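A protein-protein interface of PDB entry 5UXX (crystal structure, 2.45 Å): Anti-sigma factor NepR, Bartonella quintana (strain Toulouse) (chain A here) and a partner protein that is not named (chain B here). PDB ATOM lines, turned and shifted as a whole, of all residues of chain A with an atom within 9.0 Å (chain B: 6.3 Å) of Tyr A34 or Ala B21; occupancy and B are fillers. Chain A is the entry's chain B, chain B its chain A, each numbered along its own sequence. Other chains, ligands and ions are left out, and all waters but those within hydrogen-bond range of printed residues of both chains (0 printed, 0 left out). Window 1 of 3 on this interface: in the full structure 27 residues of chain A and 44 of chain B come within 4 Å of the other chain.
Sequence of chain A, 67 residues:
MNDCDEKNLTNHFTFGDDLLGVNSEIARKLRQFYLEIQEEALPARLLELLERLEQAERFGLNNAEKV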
ATOM      1  N   ALA A  27     -36.848 -19.113  -2.852  1.00  0.00           N
ATOM      2  CA  ALA A  27     -36.476 -17.710  -2.978  1.00  0.00           C
ATOM      3  C   ALA A  27     -35.316 -17.391  -2.045  1.00  0.00           C
ATOM      4  O   ALA A  27     -34.433 -16.601  -2.376  1.00  0.00           O
ATOM      5  CB  ALA A  27     -37.665 -16.810  -2.678  1.00  0.00           C
ATOM      6  N   ARG A  28     -35.328 -18.017  -0.873  1.00  0.00           N
ATOM      7  CA  ARG A  28     -34.266 -17.837   0.105  1.00  0.00           C
ATOM      8  C   ARG A  28     -32.973 -18.506  -0.352  1.00  0.00           C
ATOM      9  O   ARG A  28     -31.894 -17.930  -0.228  1.00  0.00           O
ATOM     10  CB  ARG A  28     -34.698 -18.388   1.464  1.00  0.00           C
ATOM     11  CG  ARG A  28     -35.533 -17.413   2.276  1.00  0.00           C
ATOM     12  CD  ARG A  28     -36.575 -18.129   3.120  1.00  0.00           C
ATOM     13  NE  ARG A  28     -37.431 -17.185   3.832  1.00  0.00           N
ATOM     14  CZ  ARG A  28     -38.441 -16.522   3.277  1.00  0.00           C
ATOM     15  NH1 ARG A  28     -38.731 -16.698   1.995  1.00  0.00           N
ATOM     16  NH2 ARG A  28     -39.163 -15.680   4.005  1.00  0.00           N
ATOM     17  N   LYS A  29     -33.090 -19.717  -0.891  1.00  0.00           N
ATOM     18  CA  LYS A  29     -31.925 -20.466  -1.352  1.00  0.00           C
ATOM     19  C   LYS A  29     -31.221 -19.768  -2.511  1.00  0.00           C
ATOM     20  O   LYS A  29     -29.998 -19.832  -2.633  1.00  0.00           O
ATOM     21  CB  LYS A  29     -32.326 -21.884  -1.764  1.00  0.00           C
ATOM     22  CG  LYS A  29     -32.596 -22.816  -0.594  1.00  0.00           C
ATOM     23  CD  LYS A  29     -33.006 -24.200  -1.070  1.00  0.00           C
ATOM     24  CE  LYS A  29     -33.227 -25.143   0.101  1.00  0.00           C
ATOM     25  NZ  LYS A  29     -32.014 -25.273   0.955  1.00  0.00           N
ATOM     26  N   LEU A  30     -31.997 -19.101  -3.360  1.00  0.00           N
ATOM     27  CA  LEU A  30     -31.435 -18.344  -4.473  1.00  0.00           C
ATOM     28  C   LEU A  30     -30.580 -17.188  -3.965  1.00  0.00           C
ATOM     29  O   LEU A  30     -29.493 -16.935  -4.484  1.00  0.00           O
ATOM     30  CB  LEU A  30     -32.545 -17.825  -5.389  1.00  0.00           C
ATOM     31  CG  LEU A  30     -33.166 -18.862  -6.329  1.00  0.00           C
ATOM     32  CD1 LEU A  30     -34.545 -18.419  -6.793  1.00  0.00           C
ATOM     33  CD2 LEU A  30     -32.253 -19.116  -7.520  1.00  0.00           C
ATOM     34  N   ARG A  31     -31.077 -16.489  -2.949  1.00  0.00           N
ATOM     35  CA  ARG A  31     -30.324 -15.403  -2.332  1.00  0.00           C
ATOM     36  C   ARG A  31     -29.092 -15.931  -1.601  1.00  0.00           C
ATOM     37  O   ARG A  31     -28.032 -15.307  -1.628  1.00  0.00           O
ATOM     38  CB  ARG A  31     -31.209 -14.609  -1.366  1.00  0.00           C
ATOM     39  CG  ARG A  31     -32.348 -13.860  -2.040  1.00  0.00           C
ATOM     40  CD  ARG A  31     -32.942 -12.806  -1.116  1.00  0.00           C
ATOM     41  NE  ARG A  31     -33.671 -13.395   0.003  1.00  0.00           N
ATOM     42  CZ  ARG A  31     -34.980 -13.626   0.007  1.00  0.00           C
ATOM     43  NH1 ARG A  31     -35.713 -13.316  -1.053  1.00  0.00           N
ATOM     44  NH2 ARG A  31     -35.557 -14.164   1.072  1.00  0.00           N
ATOM     45  N   GLN A  32     -29.240 -17.083  -0.950  1.00  0.00           N
ATOM     46  CA  GLN A  32     -28.135 -17.706  -0.227  1.00  0.00           C
ATOM     47  C   GLN A  32     -27.010 -18.108  -1.173  1.00  0.00           C
ATOM     48  O   GLN A  32     -25.842 -17.819  -0.919  1.00  0.00           O
ATOM     49  CB  GLN A  32     -28.621 -18.930   0.554  1.00  0.00           C
ATOM     50  CG  GLN A  32     -29.537 -18.606   1.722  1.00  0.00           C
ATOM     51  CD  GLN A  32     -30.367 -19.799   2.153  1.00  0.00           C
ATOM     52  OE1 GLN A  32     -30.113 -20.929   1.737  1.00  0.00           O
ATOM     53  NE2 GLN A  32     -31.368 -19.552   2.990  1.00  0.00           N
ATOM     54  N   PHE A  33     -27.374 -18.773  -2.265  1.00  0.00           N
ATOM     55  CA  PHE A  33     -26.408 -19.193  -3.274  1.00  0.00           C
ATOM     56  C   PHE A  33     -25.625 -18.005  -3.817  1.00  0.00           C
ATOM     57  O   PHE A  33     -24.405 -18.063  -3.960  1.00  0.00           O
ATOM     58  CB  PHE A  33     -27.117 -19.919  -4.420  1.00  0.00           C
ATOM     59  CG  PHE A  33     -26.193 -20.381  -5.510  1.00  0.00           C
ATOM     60  CD1 PHE A  33     -25.422 -21.522  -5.349  1.00  0.00           C
ATOM     61  CD2 PHE A  33     -26.100 -19.678  -6.701  1.00  0.00           C
ATOM     62  CE1 PHE A  33     -24.574 -21.950  -6.354  1.00  0.00           C
ATOM     63  CE2 PHE A  33     -25.254 -20.101  -7.709  1.00  0.00           C
ATOM     64  CZ  PHE A  33     -24.490 -21.239  -7.535  1.00  0.00           C
ATOM     65  N   TYR A  34     -26.341 -16.926  -4.105  1.00  0.00           N
ATOM     66  CA  TYR A  34     -25.736 -15.722  -4.655  1.00  0.00           C
ATOM     67  C   TYR A  34     -24.784 -15.084  -3.644  1.00  0.00           C
ATOM     68  O   TYR A  34     -23.727 -14.570  -4.010  1.00  0.00           O
ATOM     69  CB  TYR A  34     -26.825 -14.734  -5.072  1.00  0.00           C
ATOM     70  CG  TYR A  34     -26.500 -13.938  -6.315  1.00  0.00           C
ATOM     71  CD1 TYR A  34     -26.317 -14.574  -7.536  1.00  0.00           C
ATOM     72  CD2 TYR A  34     -26.403 -12.555  -6.277  1.00  0.00           C
ATOM     73  CE1 TYR A  34     -26.031 -13.857  -8.681  1.00  0.00           C
ATOM     74  CE2 TYR A  34     -26.119 -11.828  -7.417  1.00  0.00           C
ATOM     75  CZ  TYR A  34     -25.933 -12.484  -8.615  1.00  0.00           C
ATOM     76  OH  TYR A  34     -25.648 -11.766  -9.753  1.00  0.00           O
ATOM     77  N   LEU A  35     -25.165 -15.124  -2.370  1.00  0.00           N
ATOM     78  CA  LEU A  35     -24.347 -14.553  -1.302  1.00  0.00           C
ATOM     79  C   LEU A  35     -23.081 -15.366  -1.043  1.00  0.00           C
ATOM     80  O   LEU A  35     -21.998 -14.803  -0.889  1.00  0.00           O
ATOM     81  CB  LEU A  35     -25.163 -14.435  -0.011  1.00  0.00           C
ATOM     82  CG  LEU A  35     -24.430 -13.899   1.225  1.00  0.00           C
ATOM     83  CD1 LEU A  35     -25.287 -12.874   1.949  1.00  0.00           C
ATOM     84  CD2 LEU A  35     -24.046 -15.030   2.174  1.00  0.00           C
ATOM     85  N   GLU A  36     -23.223 -16.687  -0.990  1.00  0.00           N
ATOM     86  CA  GLU A  36     -22.098 -17.566  -0.684  1.00  0.00           C
ATOM     87  C   GLU A  36     -21.002 -17.484  -1.743  1.00  0.00           C
ATOM     88  O   GLU A  36     -19.817 -17.586  -1.429  1.00  0.00           O
ATOM     89  CB  GLU A  36     -22.573 -19.014  -0.536  1.00  0.00           C
ATOM     90  CG  GLU A  36     -23.520 -19.258   0.634  1.00  0.00           C
ATOM     91  CD  GLU A  36     -22.826 -19.263   1.988  1.00  0.00           C
ATOM     92  OE1 GLU A  36     -21.633 -18.903   2.068  1.00  0.00           O
ATOM     93  OE2 GLU A  36     -23.486 -19.632   2.982  1.00  0.00           O
ATOM     94  N   ILE A  37     -21.403 -17.306  -2.999  1.00  0.00           N
ATOM     95  CA  ILE A  37     -20.448 -17.143  -4.089  1.00  0.00           C
ATOM     96  C   ILE A  37     -19.623 -15.873  -3.891  1.00  0.00           C
ATOM     97  O   ILE A  37     -18.417 -15.854  -4.142  1.00  0.00           O
ATOM     98  CB  ILE A  37     -21.155 -17.092  -5.458  1.00  0.00           C
ATOM     99  CG1 ILE A  37     -21.831 -18.431  -5.759  1.00  0.00           C
ATOM    100  CG2 ILE A  37     -20.169 -16.758  -6.559  1.00  0.00           C
ATOM    101  CD1 ILE A  37     -20.880 -19.606  -5.768  1.00  0.00           C
ATOM    102  N   GLN A  38     -20.280 -14.818  -3.420  1.00  0.00           N
ATOM    103  CA  GLN A  38     -19.620 -13.535  -3.207  1.00  0.00           C
ATOM    104  C   GLN A  38     -18.811 -13.514  -1.910  1.00  0.00           C
ATOM    105  O   GLN A  38     -18.058 -12.573  -1.658  1.00  0.00           O
ATOM    106  CB  GLN A  38     -20.650 -12.404  -3.208  1.00  0.00           C
ATOM    107  CG  GLN A  38     -21.411 -12.273  -4.518  1.00  0.00           C
ATOM    108  CD  GLN A  38     -22.411 -11.133  -4.503  1.00  0.00           C
ATOM    109  OE1 GLN A  38     -22.033  -9.962  -4.486  1.00  0.00           O
ATOM    110  NE2 GLN A  38     -23.694 -11.472  -4.509  1.00  0.00           N
ATOM    111  N   GLU A  39     -18.974 -14.545  -1.088  1.00  0.00           N
ATOM    112  CA  GLU A  39     -18.149 -14.698   0.108  1.00  0.00           C
ATOM    113  C   GLU A  39     -16.703 -14.969  -0.288  1.00  0.00           C
ATOM    114  O   GLU A  39     -15.769 -14.572   0.409  1.00  0.00           O
ATOM    115  CB  GLU A  39     -18.670 -15.834   0.993  1.00  0.00           C
ATOM    116  CG  GLU A  39     -19.920 -15.498   1.786  1.00  0.00           C
ATOM    117  CD  GLU A  39     -19.642 -14.546   2.931  1.00  0.00           C
ATOM    118  OE1 GLU A  39     -18.680 -14.795   3.688  1.00  0.00           O
ATOM    119  OE2 GLU A  39     -20.383 -13.551   3.074  1.00  0.00           O
ATOM    120  N   GLU A  40     -16.533 -15.648  -1.417  1.00  0.00           N
ATOM    121  CA  GLU A  40     -15.210 -15.983  -1.928  1.00  0.00           C
ATOM    122  C   GLU A  40     -14.452 -14.736  -2.374  1.00  0.00           C
ATOM    123  O   GLU A  40     -15.054 -13.735  -2.764  1.00  0.00           O
ATOM    124  CB  GLU A  40     -15.327 -16.978  -3.085  1.00  0.00           C
ATOM    125  CG  GLU A  40     -16.115 -18.232  -2.736  1.00  0.00           C
ATOM    126  CD  GLU A  40     -16.356 -19.132  -3.933  1.00  0.00           C
ATOM    127  OE1 GLU A  40     -16.289 -18.636  -5.079  1.00  0.00           O
ATOM    128  OE2 GLU A  40     -16.614 -20.337  -3.728  1.00  0.00           O
ATOM    129  N   LEU A  42     -12.478 -12.063  -4.457  1.00  0.00           N
ATOM    130  CA  LEU A  42     -12.444 -11.592  -5.833  1.00  0.00           C
ATOM    131  C   LEU A  42     -11.001 -11.636  -6.322  1.00  0.00           C
ATOM    132  O   LEU A  42     -10.134 -10.977  -5.748  1.00  0.00           O
ATOM    133  CB  LEU A  42     -13.012 -10.177  -5.944  1.00  0.00           C
ATOM    134  CG  LEU A  42     -13.501  -9.759  -7.332  1.00  0.00           C
ATOM    135  CD1 LEU A  42     -14.827 -10.432  -7.655  1.00  0.00           C
ATOM    136  CD2 LEU A  42     -13.626  -8.253  -7.430  1.00  0.00           C
ATOM    137  N   PRO A  43     -10.740 -12.428  -7.377  1.00  0.00           N
ATOM    138  CA  PRO A  43      -9.393 -12.706  -7.894  1.00  0.00           C
ATOM    139  C   PRO A  43      -8.554 -11.449  -8.104  1.00  0.00           C
ATOM    140  O   PRO A  43      -9.033 -10.471  -8.679  1.00  0.00           O
ATOM    141  CB  PRO A  43      -9.673 -13.396  -9.232  1.00  0.00           C
ATOM    142  CG  PRO A  43     -11.000 -14.034  -9.048  1.00  0.00           C
ATOM    143  CD  PRO A  43     -11.784 -13.094  -8.177  1.00  0.00           C
ATOM    144  N   LEU A  46      -8.156  -9.791 -11.499  1.00  0.00           N
ATOM    145  CA  LEU A  46      -9.308  -9.005 -11.918  1.00  0.00           C
ATOM    146  C   LEU A  46      -9.186  -7.568 -11.422  1.00  0.00           C
ATOM    147  O   LEU A  46      -9.469  -6.621 -12.156  1.00  0.00           O
ATOM    148  CB  LEU A  46     -10.601  -9.640 -11.407  1.00  0.00           C
ATOM    149  CG  LEU A  46     -11.910  -9.057 -11.935  1.00  0.00           C
ATOM    150  CD1 LEU A  46     -11.984  -9.196 -13.447  1.00  0.00           C
ATOM    151  CD2 LEU A  46     -13.095  -9.738 -11.270  1.00  0.00           C
ATOM    152  N   LEU B  16     -18.869  -5.632  -9.470  1.00  0.00           N
ATOM    153  CA  LEU B  16     -17.963  -6.735  -9.790  1.00  0.00           C
ATOM    154  C   LEU B  16     -18.235  -8.052  -9.033  1.00  0.00           C
ATOM    155  O   LEU B  16     -18.183  -9.121  -9.642  1.00  0.00           O
ATOM    156  CB  LEU B  16     -16.513  -6.293  -9.564  1.00  0.00           C
ATOM    157  CG  LEU B  16     -15.445  -7.024 -10.376  1.00  0.00           C
ATOM    158  CD1 LEU B  16     -15.949  -7.325 -11.779  1.00  0.00           C
ATOM    159  CD2 LEU B  16     -14.167  -6.202 -10.434  1.00  0.00           C
ATOM    160  N   PRO B  17     -18.517  -7.992  -7.714  1.00  0.00           N
ATOM    161  CA  PRO B  17     -18.816  -9.262  -7.037  1.00  0.00           C
ATOM    162  C   PRO B  17     -20.080  -9.950  -7.553  1.00  0.00           C
ATOM    163  O   PRO B  17     -20.094 -11.172  -7.700  1.00  0.00           O
ATOM    164  CB  PRO B  17     -18.999  -8.845  -5.574  1.00  0.00           C
ATOM    165  CG  PRO B  17     -18.226  -7.593  -5.442  1.00  0.00           C
ATOM    166  CD  PRO B  17     -18.408  -6.884  -6.747  1.00  0.00           C
ATOM    167  N   ALA B  18     -21.125  -9.173  -7.818  1.00  0.00           N
ATOM    168  CA  ALA B  18     -22.373  -9.728  -8.331  1.00  0.00           C
ATOM    169  C   ALA B  18     -22.193 -10.204  -9.766  1.00  0.00           C
ATOM    170  O   ALA B  18     -22.799 -11.190 -10.186  1.00  0.00           O
ATOM    171  CB  ALA B  18     -23.489  -8.699  -8.247  1.00  0.00           C
ATOM    172  N   LEU B  19     -21.361  -9.487 -10.515  1.00  0.00           N
ATOM    173  CA  LEU B  19     -21.051  -9.846 -11.892  1.00  0.00           C
ATOM    174  C   LEU B  19     -20.367 -11.209 -11.956  1.00  0.00           C
ATOM    175  O   LEU B  19     -20.655 -12.021 -12.837  1.00  0.00           O
ATOM    176  CB  LEU B  19     -20.164  -8.778 -12.534  1.00  0.00           C
ATOM    177  CG  LEU B  19     -19.923  -8.898 -14.038  1.00  0.00           C
ATOM    178  CD1 LEU B  19     -21.219  -8.680 -14.806  1.00  0.00           C
ATOM    179  CD2 LEU B  19     -18.855  -7.915 -14.489  1.00  0.00           C
ATOM    180  N   ARG B  20     -19.459 -11.452 -11.015  1.00  0.00           N
ATOM    181  CA  ARG B  20     -18.755 -12.725 -10.933  1.00  0.00           C
ATOM    182  C   ARG B  20     -19.701 -13.859 -10.549  1.00  0.00           C
ATOM    183  O   ARG B  20     -19.613 -14.963 -11.089  1.00  0.00           O
ATOM    184  CB  ARG B  20     -17.604 -12.636  -9.928  1.00  0.00           C
ATOM    185  CG  ARG B  20     -16.880 -13.953  -9.693  1.00  0.00           C
ATOM    186  CD  ARG B  20     -15.718 -13.780  -8.730  1.00  0.00           C
ATOM    187  NE  ARG B  20     -15.168 -15.061  -8.297  1.00  0.00           N
ATOM    188  CZ  ARG B  20     -15.631 -15.762  -7.268  1.00  0.00           C
ATOM    189  NH1 ARG B  20     -16.653 -15.307  -6.558  1.00  0.00           N
ATOM    190  NH2 ARG B  20     -15.069 -16.920  -6.947  1.00  0.00           N
ATOM    191  N   ALA B  21     -20.603 -13.580  -9.612  1.00  0.00           N
ATOM    192  CA  ALA B  21     -21.591 -14.562  -9.175  1.00  0.00           C
ATOM    193  C   ALA B  21     -22.521 -14.945 -10.321  1.00  0.00           C
ATOM    194  O   ALA B  21     -22.951 -16.094 -10.431  1.00  0.00           O
ATOM    195  CB  ALA B  21     -22.392 -14.026  -7.999  1.00  0.00           C
ATOM    196  N   PHE B  22     -22.827 -13.969 -11.169  1.00  0.00           N
ATOM    197  CA  PHE B  22     -23.669 -14.193 -12.337  1.00  0.00           C
ATOM    198  C   PHE B  22     -22.983 -15.122 -13.330  1.00  0.00           C
ATOM    199  O   PHE B  22     -23.613 -16.015 -13.897  1.00  0.00           O
ATOM    200  CB  PHE B  22     -24.016 -12.861 -13.006  1.00  0.00           C
ATOM    201  CG  PHE B  22     -24.931 -12.992 -14.190  1.00  0.00           C
ATOM    202  CD1 PHE B  22     -26.148 -13.644 -14.075  1.00  0.00           C
ATOM    203  CD2 PHE B  22     -24.579 -12.450 -15.416  1.00  0.00           C
ATOM    204  CE1 PHE B  22     -26.993 -13.762 -15.164  1.00  0.00           C
ATOM    205  CE2 PHE B  22     -25.420 -12.564 -16.509  1.00  0.00           C
ATOM    206  CZ  PHE B  22     -26.630 -13.221 -16.382  1.00  0.00           C
ATOM    207  N   ALA B  23     -21.687 -14.906 -13.533  1.00  0.00           N
ATOM    208  CA  ALA B  23     -20.904 -15.717 -14.457  1.00  0.00           C
ATOM    209  C   ALA B  23     -20.813 -17.166 -13.989  1.00  0.00           C
ATOM    210  O   ALA B  23     -20.945 -18.093 -14.788  1.00  0.00           O
ATOM    211  CB  ALA B  23     -19.512 -15.130 -14.625  1.00  0.00           C
ATOM    212  N   ILE B  24     -20.586 -17.354 -12.694  1.00  0.00           N
ATOM    213  CA  ILE B  24     -20.478 -18.689 -12.118  1.00  0.00           C
ATOM    214  C   ILE B  24     -21.818 -19.422 -12.192  1.00  0.00           C
ATOM    215  O   ILE B  24     -21.870 -20.610 -12.513  1.00  0.00           O
ATOM    216  CB  ILE B  24     -19.987 -18.627 -10.655  1.00  0.00           C
ATOM    217  CG1 ILE B  24     -18.516 -18.207 -10.613  1.00  0.00           C
ATOM    218  CG2 ILE B  24     -20.169 -19.968  -9.960  1.00  0.00           C
ATOM    219  CD1 ILE B  24     -18.008 -17.874  -9.228  1.00  0.00           C
ATOM    220  N   SER B  25     -22.899 -18.701 -11.912  1.00  0.00           N
ATOM    221  CA  SER B  25     -24.243 -19.266 -11.990  1.00  0.00           C
ATOM    222  C   SER B  25     -24.594 -19.671 -13.418  1.00  0.00           C
ATOM    223  O   SER B  25     -25.307 -20.649 -13.644  1.00  0.00           O
ATOM    224  CB  SER B  25     -25.275 -18.266 -11.464  1.00  0.00           C
ATOM    225  OG  SER B  25     -24.992 -17.889 -10.129  1.00  0.00           O
ATOM    226  N   LEU B  26     -24.084 -18.908 -14.379  1.00  0.00           N
ATOM    227  CA  LEU B  26     -24.413 -19.100 -15.786  1.00  0.00           C
ATOM    228  C   LEU B  26     -23.570 -20.191 -16.444  1.00  0.00           C
ATOM    229  O   LEU B  26     -24.039 -20.894 -17.339  1.00  0.00           O
ATOM    230  CB  LEU B  26     -24.231 -17.783 -16.544  1.00  0.00           C
ATOM    231  CG  LEU B  26     -25.340 -17.341 -17.498  1.00  0.00           C
ATOM    232  CD1 LEU B  26     -26.682 -17.311 -16.786  1.00  0.00           C
ATOM    233  CD2 LEU B  26     -25.013 -15.977 -18.086  1.00  0.00           C
ATOM    234  N   VAL B  37     -15.650 -13.070 -16.749  1.00  0.00           N
ATOM    235  CA  VAL B  37     -15.713 -11.791 -16.051  1.00  0.00           C
ATOM    236  C   VAL B  37     -14.625 -10.850 -16.561  1.00  0.00           C
ATOM    237  O   VAL B  37     -14.873  -9.667 -16.799  1.00  0.00           O
ATOM    238  CB  VAL B  37     -15.560 -11.972 -14.530  1.00  0.00           C
ATOM    239  CG1 VAL B  37     -15.605 -10.625 -13.827  1.00  0.00           C
ATOM    240  CG2 VAL B  37     -16.646 -12.888 -13.995  1.00  0.00           C
ATOM    241  N   PHE B  62     -24.305  -6.771 -17.036  1.00  0.00           N
ATOM    242  CA  PHE B  62     -24.786  -8.145 -17.118  1.00  0.00           C
ATOM    243  C   PHE B  62     -25.099  -8.539 -18.558  1.00  0.00           C
ATOM    244  O   PHE B  62     -24.902  -9.688 -18.952  1.00  0.00           O
ATOM    245  CB  PHE B  62     -26.027  -8.336 -16.243  1.00  0.00           C
ATOM    246  CG  PHE B  62     -25.717  -8.662 -14.806  1.00  0.00           C
ATOM    247  CD1 PHE B  62     -24.804  -7.909 -14.085  1.00  0.00           C
ATOM    248  CD2 PHE B  62     -26.349  -9.722 -14.174  1.00  0.00           C
ATOM    249  CE1 PHE B  62     -24.523  -8.209 -12.764  1.00  0.00           C
ATOM    250  CE2 PHE B  62     -26.074 -10.026 -12.852  1.00  0.00           C
ATOM    251  CZ  PHE B  62     -25.159  -9.270 -12.148  1.00  0.00           C
ATOM    252  N   LEU B 101     -25.992 -23.868   2.988  1.00  0.00           N
ATOM    253  CA  LEU B 101     -26.477 -24.294   1.679  1.00  0.00           C
ATOM    254  C   LEU B 101     -25.437 -25.114   0.922  1.00  0.00           C
ATOM    255  O   LEU B 101     -24.286 -24.700   0.783  1.00  0.00           O
ATOM    256  CB  LEU B 101     -26.890 -23.086   0.835  1.00  0.00           C
ATOM    257  CG  LEU B 101     -27.434 -23.428  -0.555  1.00  0.00           C
ATOM    258  CD1 LEU B 101     -28.756 -24.175  -0.447  1.00  0.00           C
ATOM    259  CD2 LEU B 101     -27.586 -22.177  -1.407  1.00  0.00           C
ATOM    260  N   LEU B 103     -23.786 -25.720  -1.966  1.00  0.00           N
ATOM    261  CA  LEU B 103     -23.593 -24.947  -3.189  1.00  0.00           C
ATOM    262  C   LEU B 103     -23.398 -25.841  -4.406  1.00  0.00           C
ATOM    263  O   LEU B 103     -23.890 -25.538  -5.492  1.00  0.00           O
ATOM    264  CB  LEU B 103     -22.394 -24.009  -3.041  1.00  0.00           C
ATOM    265  CG  LEU B 103     -22.475 -22.996  -1.900  1.00  0.00           C
ATOM    266  CD1 LEU B 103     -21.222 -22.136  -1.864  1.00  0.00           C
ATOM    267  CD2 LEU B 103     -23.721 -22.134  -2.043  1.00  0.00           C
ATOM    268  N   ILE B 122     -32.013 -16.653 -12.138  1.00  0.00           N
ATOM    269  CA  ILE B 122     -30.855 -16.001 -11.531  1.00  0.00           C
ATOM    270  C   ILE B 122     -31.019 -14.484 -11.557  1.00  0.00           C
ATOM    271  O   ILE B 122     -30.797 -13.811 -10.551  1.00  0.00           O
ATOM    272  CB  ILE B 122     -29.543 -16.395 -12.241  1.00  0.00           C
ATOM    273  CG1 ILE B 122     -29.189 -17.851 -11.931  1.00  0.00           C
ATOM    274  CG2 ILE B 122     -28.402 -15.492 -11.803  1.00  0.00           C
ATOM    275  CD1 ILE B 122     -29.049 -18.143 -10.452  1.00  0.00           C
ATOM    276  N   ALA B 126     -32.063 -13.837  -7.885  1.00  0.00           N
ATOM    277  CA  ALA B 126     -30.777 -13.659  -7.219  1.00  0.00           C
ATOM    278  C   ALA B 126     -30.118 -12.311  -7.509  1.00  0.00           C
ATOM    279  O   ALA B 126     -29.525 -11.704  -6.618  1.00  0.00           O
ATOM    280  CB  ALA B 126     -29.835 -14.789  -7.608  1.00  0.00           C
ATOM    281  N   SER B 127     -30.219 -11.846  -8.749  1.00  0.00           N
ATOM    282  CA  SER B 127     -29.506 -10.640  -9.164  1.00  0.00           C
ATOM    283  C   SER B 127     -30.267  -9.361  -8.820  1.00  0.00           C
ATOM    284  O   SER B 127     -29.709  -8.265  -8.879  1.00  0.00           O
ATOM    285  CB  SER B 127     -29.216 -10.688 -10.665  1.00  0.00           C
ATOM    286  OG  SER B 127     -28.492 -11.859 -11.001  1.00  0.00           O
ATOM    287  N   GLY B 128     -31.540  -9.501  -8.468  1.00  0.00           N
ATOM    288  CA  GLY B 128     -32.325  -8.374  -7.998  1.00  0.00           C
ATOM    289  C   GLY B 128     -32.868  -7.461  -9.083  1.00  0.00           C
ATOM    290  O   GLY B 128     -33.200  -6.307  -8.815  1.00  0.00           O
ATOM    291  N   PHE B 129     -32.957  -7.970 -10.308  1.00  0.00           N
ATOM    292  CA  PHE B 129     -33.513  -7.188 -11.410  1.00  0.00           C
ATOM    293  C   PHE B 129     -35.036  -7.245 -11.430  1.00  0.00           C
ATOM    294  O   PHE B 129     -35.638  -8.215 -10.969  1.00  0.00           O
ATOM    295  CB  PHE B 129     -32.966  -7.675 -12.754  1.00  0.00           C
ATOM    296  CG  PHE B 129     -31.512  -7.373 -12.967  1.00  0.00           C
ATOM    297  CD1 PHE B 129     -31.086  -6.071 -13.176  1.00  0.00           C
ATOM    298  CD2 PHE B 129     -30.574  -8.390 -12.972  1.00  0.00           C
ATOM    299  CE1 PHE B 129     -29.749  -5.789 -13.375  1.00  0.00           C
ATOM    300  CE2 PHE B 129     -29.234  -8.115 -13.172  1.00  0.00           C
ATOM    301  CZ  PHE B 129     -28.821  -6.814 -13.374  1.00  0.00           C
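Of the 17 printed residues of chain A, 12 touch a printed residue of chain B.
Printed residues of chain A that touch a printed residue of chain B: Lys A29, Leu A30, Gln A32, Phe A33, Tyr A34, Glu A36, Ile A37, Gln A38, Glu A40, Leu A42, Pro A43 and Leu A46.
Hydrophobic or aromatic side chains of chain B that line the printed part of chain A: Leu B16, Pro B17, Ala B21, Phe B22, Ile B24, Val B37, Phe B62, Leu B101, Leu B103 and Ala B126.
Tyr A34 touches just these residues of chain B: Ala B18 (2.9 Å), Ala B21 (3.7 Å), Phe B22 (3.8 Å), Phe B62 (3.5 Å), Ala B126 (3.3 Å) and Ser B127 (3.1 Å).
Printed residues of chain B within 4 Å of Glu A36: Leu B103.
Glu A39 touches none of the printed residues of chain B.
Of the printed residues of chain A, Ala B21 touches Tyr A34 (3.7 Å) and Ile A37 (3.7 Å).
Ala B23 touches none of the printed residues of chain A.
Printed residues of chain A within 4 Å of Leu B103: Phe A33 and Glu A36.
The nearest residue of chain B that does not touch Tyr A34 is Ile B122 (4.2 Å).
The nearest printed residue of chain A that does not touch Phe B22 is Ile A37 (6.0 Å).
The side-chain hydroxyl of Ser B25 lies within hydrogen-bond range of the backbone carbonyl oxygen of Ala B21 (2.7 Å).
The backbone NH (N) of Ser B127 is in hydrogen-bond range of the backbone carbonyl oxygen (O) of Ile B122 (2.7 Å).
The backbone carbonyl oxygen of Tyr A34 sits at hydrogen-bond distance from the side-chain amide nitrogen of Gln A38 (3.1 Å).
CD2 of Leu B101 touches CB of Gln A32, 3.9 Å away.
Phe A33 touches Ser B25.
N of Phe A33 touches CD2 of Leu B101 (3.5 Å).
Tyr A34 touches Phe B62 (OH to CZ, 3.5 Å).
Ala B126 touches Tyr A34 (O to CD2, 3.3 Å).
Ala B21 touches Ile A37 (CA to CG2, 3.7 Å).
Pro B17 touches Gln A38 (CB to OE1, 3.4 Å).
Gln A38 touches Ala B18 (OE1 to N, 3.5 Å).
Pro A43 touches Arg B20.
Leu A46 touches Val B37 (CD2 to CG1, 3.7 Å).
The side-chain hydroxyl (OH) of Tyr A34 is in hydrogen-bond range of the backbone carbonyl oxygen (O) of Ala B18.
The guanidinium group (NH1) of Arg B20 lies within hydrogen-bond range of the backbone carbonyl oxygen (O) of Ile A37 (3.0 Å).
NH2 of Arg B20 lies within salt-bridge range of OE1 of Glu A40 (2.8 Å).
OG of Ser B127 sits at hydrogen-bond distance from OH of Tyr A34, 3.1 Å away.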
